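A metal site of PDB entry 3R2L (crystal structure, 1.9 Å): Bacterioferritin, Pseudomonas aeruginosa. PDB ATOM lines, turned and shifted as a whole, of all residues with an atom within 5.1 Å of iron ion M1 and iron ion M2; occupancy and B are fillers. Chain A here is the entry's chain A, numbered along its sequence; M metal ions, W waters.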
ATOM      1  N   GLU A  18      13.309   8.765 -27.075  1.00  0.00           N
ATOM      2  CA  GLU A  18      13.517   8.972 -25.614  1.00  0.00           C
ATOM      3  C   GLU A  18      13.412   7.632 -24.853  1.00  0.00           C
ATOM      4  O   GLU A  18      14.192   7.380 -23.915  1.00  0.00           O
ATOM      5  CB  GLU A  18      12.494   9.981 -25.026  1.00  0.00           C
ATOM      6  CG  GLU A  18      12.622  11.337 -25.663  1.00  0.00           C
ATOM      7  CD  GLU A  18      14.006  11.934 -25.462  1.00  0.00           C
ATOM      8  OE1 GLU A  18      14.448  12.004 -24.319  1.00  0.00           O
ATOM      9  OE2 GLU A  18      14.664  12.307 -26.435  1.00  0.00           O
ATOM     10  N   TYR A  25      20.741   4.187 -21.207  1.00  0.00           N
ATOM     11  CA  TYR A  25      21.271   4.561 -19.879  1.00  0.00           C
ATOM     12  C   TYR A  25      20.996   3.482 -18.827  1.00  0.00           C
ATOM     13  O   TYR A  25      21.808   3.295 -17.896  1.00  0.00           O
ATOM     14  CB  TYR A  25      20.600   5.852 -19.439  1.00  0.00           C
ATOM     15  CG  TYR A  25      21.122   7.070 -20.203  1.00  0.00           C
ATOM     16  CD1 TYR A  25      22.484   7.217 -20.455  1.00  0.00           C
ATOM     17  CD2 TYR A  25      20.279   8.078 -20.616  1.00  0.00           C
ATOM     18  CE1 TYR A  25      23.003   8.376 -21.089  1.00  0.00           C
ATOM     19  CE2 TYR A  25      20.771   9.214 -21.271  1.00  0.00           C
ATOM     20  CZ  TYR A  25      22.148   9.359 -21.506  1.00  0.00           C
ATOM     21  OH  TYR A  25      22.670  10.469 -22.149  1.00  0.00           O
ATOM     22  N   GLU A  51      15.399  10.702 -18.755  1.00  0.00           N
ATOM     23  CA  GLU A  51      14.819  10.344 -20.067  1.00  0.00           C
ATOM     24  C   GLU A  51      13.420   9.778 -19.899  1.00  0.00           C
ATOM     25  O   GLU A  51      12.597   9.911 -20.757  1.00  0.00           O
ATOM     26  CB  GLU A  51      15.670   9.299 -20.827  1.00  0.00           C
ATOM     27  CG  GLU A  51      17.135   9.684 -21.034  1.00  0.00           C
ATOM     28  CD  GLU A  51      17.355  10.942 -21.913  1.00  0.00           C
ATOM     29  OE1 GLU A  51      16.409  11.601 -22.325  1.00  0.00           O
ATOM     30  OE2 GLU A  51      18.503  11.244 -22.185  1.00  0.00           O
ATOM     31  N   HIS A  54      11.353  12.688 -19.851  1.00  0.00           N
ATOM     32  CA  HIS A  54      11.228  13.296 -21.190  1.00  0.00           C
ATOM     33  C   HIS A  54      10.225  12.493 -22.011  1.00  0.00           C
ATOM     34  O   HIS A  54       9.358  13.038 -22.674  1.00  0.00           O
ATOM     35  CB  HIS A  54      12.560  13.287 -21.931  1.00  0.00           C
ATOM     36  CG  HIS A  54      13.532  14.304 -21.447  1.00  0.00           C
ATOM     37  ND1 HIS A  54      14.807  14.398 -21.940  1.00  0.00           N
ATOM     38  CD2 HIS A  54      13.416  15.291 -20.524  1.00  0.00           C
ATOM     39  CE1 HIS A  54      15.451  15.376 -21.337  1.00  0.00           C
ATOM     40  NE2 HIS A  54      14.624  15.948 -20.478  1.00  0.00           N
ATOM     41  N   GLU A  93      22.833  11.366 -27.836  1.00  0.00           N
ATOM     42  CA  GLU A  93      22.358  12.705 -27.434  1.00  0.00           C
ATOM     43  C   GLU A  93      22.479  13.698 -28.602  1.00  0.00           C
ATOM     44  O   GLU A  93      21.642  14.563 -28.735  1.00  0.00           O
ATOM     45  CB  GLU A  93      23.189  13.241 -26.244  1.00  0.00           C
ATOM     46  CG  GLU A  93      22.955  12.434 -24.953  1.00  0.00           C
ATOM     47  CD  GLU A  93      21.552  12.685 -24.327  1.00  0.00           C
ATOM     48  OE1 GLU A  93      20.874  13.689 -24.651  1.00  0.00           O
ATOM     49  OE2 GLU A  93      21.147  11.880 -23.453  1.00  0.00           O
ATOM     50  N   VAL A  96      19.532  13.068 -30.736  1.00  0.00           N
ATOM     51  CA  VAL A  96      18.341  13.640 -30.089  1.00  0.00           C
ATOM     52  C   VAL A  96      18.307  15.160 -30.248  1.00  0.00           C
ATOM     53  O   VAL A  96      17.247  15.729 -30.532  1.00  0.00           O
ATOM     54  CB  VAL A  96      18.281  13.270 -28.575  1.00  0.00           C
ATOM     55  CG1 VAL A  96      17.170  14.085 -27.895  1.00  0.00           C
ATOM     56  CG2 VAL A  96      18.023  11.776 -28.422  1.00  0.00           C
ATOM     57  N   GLN A 122      13.335  20.109 -23.370  1.00  0.00           N
ATOM     58  CA  GLN A 122      14.134  18.916 -23.527  1.00  0.00           C
ATOM     59  C   GLN A 122      15.417  19.181 -24.266  1.00  0.00           C
ATOM     60  O   GLN A 122      16.430  18.555 -23.979  1.00  0.00           O
ATOM     61  CB  GLN A 122      13.302  17.835 -24.231  1.00  0.00           C
ATOM     62  CG  GLN A 122      12.188  17.367 -23.332  1.00  0.00           C
ATOM     63  CD  GLN A 122      11.436  16.166 -23.854  1.00  0.00           C
ATOM     64  OE1 GLN A 122      10.327  15.866 -23.372  1.00  0.00           O
ATOM     65  NE2 GLN A 122      12.012  15.470 -24.827  1.00  0.00           N
ATOM     66  N   THR A 126      19.163  18.308 -23.081  1.00  0.00           N
ATOM     67  CA  THR A 126      20.063  17.528 -23.943  1.00  0.00           C
ATOM     68  C   THR A 126      21.420  18.227 -24.152  1.00  0.00           C
ATOM     69  O   THR A 126      22.494  17.640 -23.954  1.00  0.00           O
ATOM     70  CB  THR A 126      19.376  17.303 -25.335  1.00  0.00           C
ATOM     71  OG1 THR A 126      18.179  16.527 -25.121  1.00  0.00           O
ATOM     72  CG2 THR A 126      20.334  16.613 -26.294  1.00  0.00           C
ATOM     73  N   HIS A 130      22.931  16.648 -20.474  1.00  0.00           N
ATOM     74  CA  HIS A 130      23.335  15.299 -20.934  1.00  0.00           C
ATOM     75  C   HIS A 130      24.578  15.317 -21.861  1.00  0.00           C
ATOM     76  O   HIS A 130      25.604  14.728 -21.545  1.00  0.00           O
ATOM     77  CB  HIS A 130      22.153  14.596 -21.639  1.00  0.00           C
ATOM     78  CG  HIS A 130      20.919  14.521 -20.787  1.00  0.00           C
ATOM     79  ND1 HIS A 130      19.751  13.910 -21.207  1.00  0.00           N
ATOM     80  CD2 HIS A 130      20.680  14.963 -19.526  1.00  0.00           C
ATOM     81  CE1 HIS A 130      18.852  13.987 -20.238  1.00  0.00           C
ATOM     82  NE2 HIS A 130      19.385  14.626 -19.216  1.00  0.00           N
HETATM   83 FE    FE M   1      15.847  13.227 -23.547  1.00  0.00          FE
HETATM   84 FE    FE M   2      19.260  12.978 -23.060  1.00  0.00          FE
HETATM   85  O   HOH W   1      15.198  14.655 -25.059  1.00  0.00           O
HETATM   86  O   HOH W   2      17.698  14.117 -23.742  1.00  0.00           O
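OE2 of Glu 93 lies close to OH of Tyr 25, at 2.5 Å. The backbone carbonyl oxygen of His 54 sits close to the side-chain amide oxygen of Gln 122 (3.1 Å).
Within 4 Å of iron ion M1: Glu 18, Glu 51 and His 54.
Within 4 Å of iron ion M2: Glu 51, Glu 93 and His 130.
OE1 of Glu 18 binds iron ion M1 (2.0 Å). Iron ion M1 is bound by water W2. The side-chain carboxylate (OE1) of Glu 51 is bound to iron ion M1 (2.1 Å). Water W1 is bound to iron ion M1, at 2.2 Å. A ring nitrogen (ND1) of His 54 is bound to iron ion M1, at 2.2 Å.
Iron ion M2 is bound by water W2 (2.0 Å), OE2 of Glu 51 (2.1 Å), ND1 of His 130 (2.1 Å), OE2 of Glu 93 (2.2 Å) and OE1 of Glu 93 (2.4 Å). Iron ion M2 has five donor atoms within binding distance.
Water W1 lies within hydrogen-bond range of the side-chain carboxylate (OE2) of Glu 18 (2.8 Å) and the side-chain amide nitrogen (NE2) of Gln 122 (3.3 Å).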
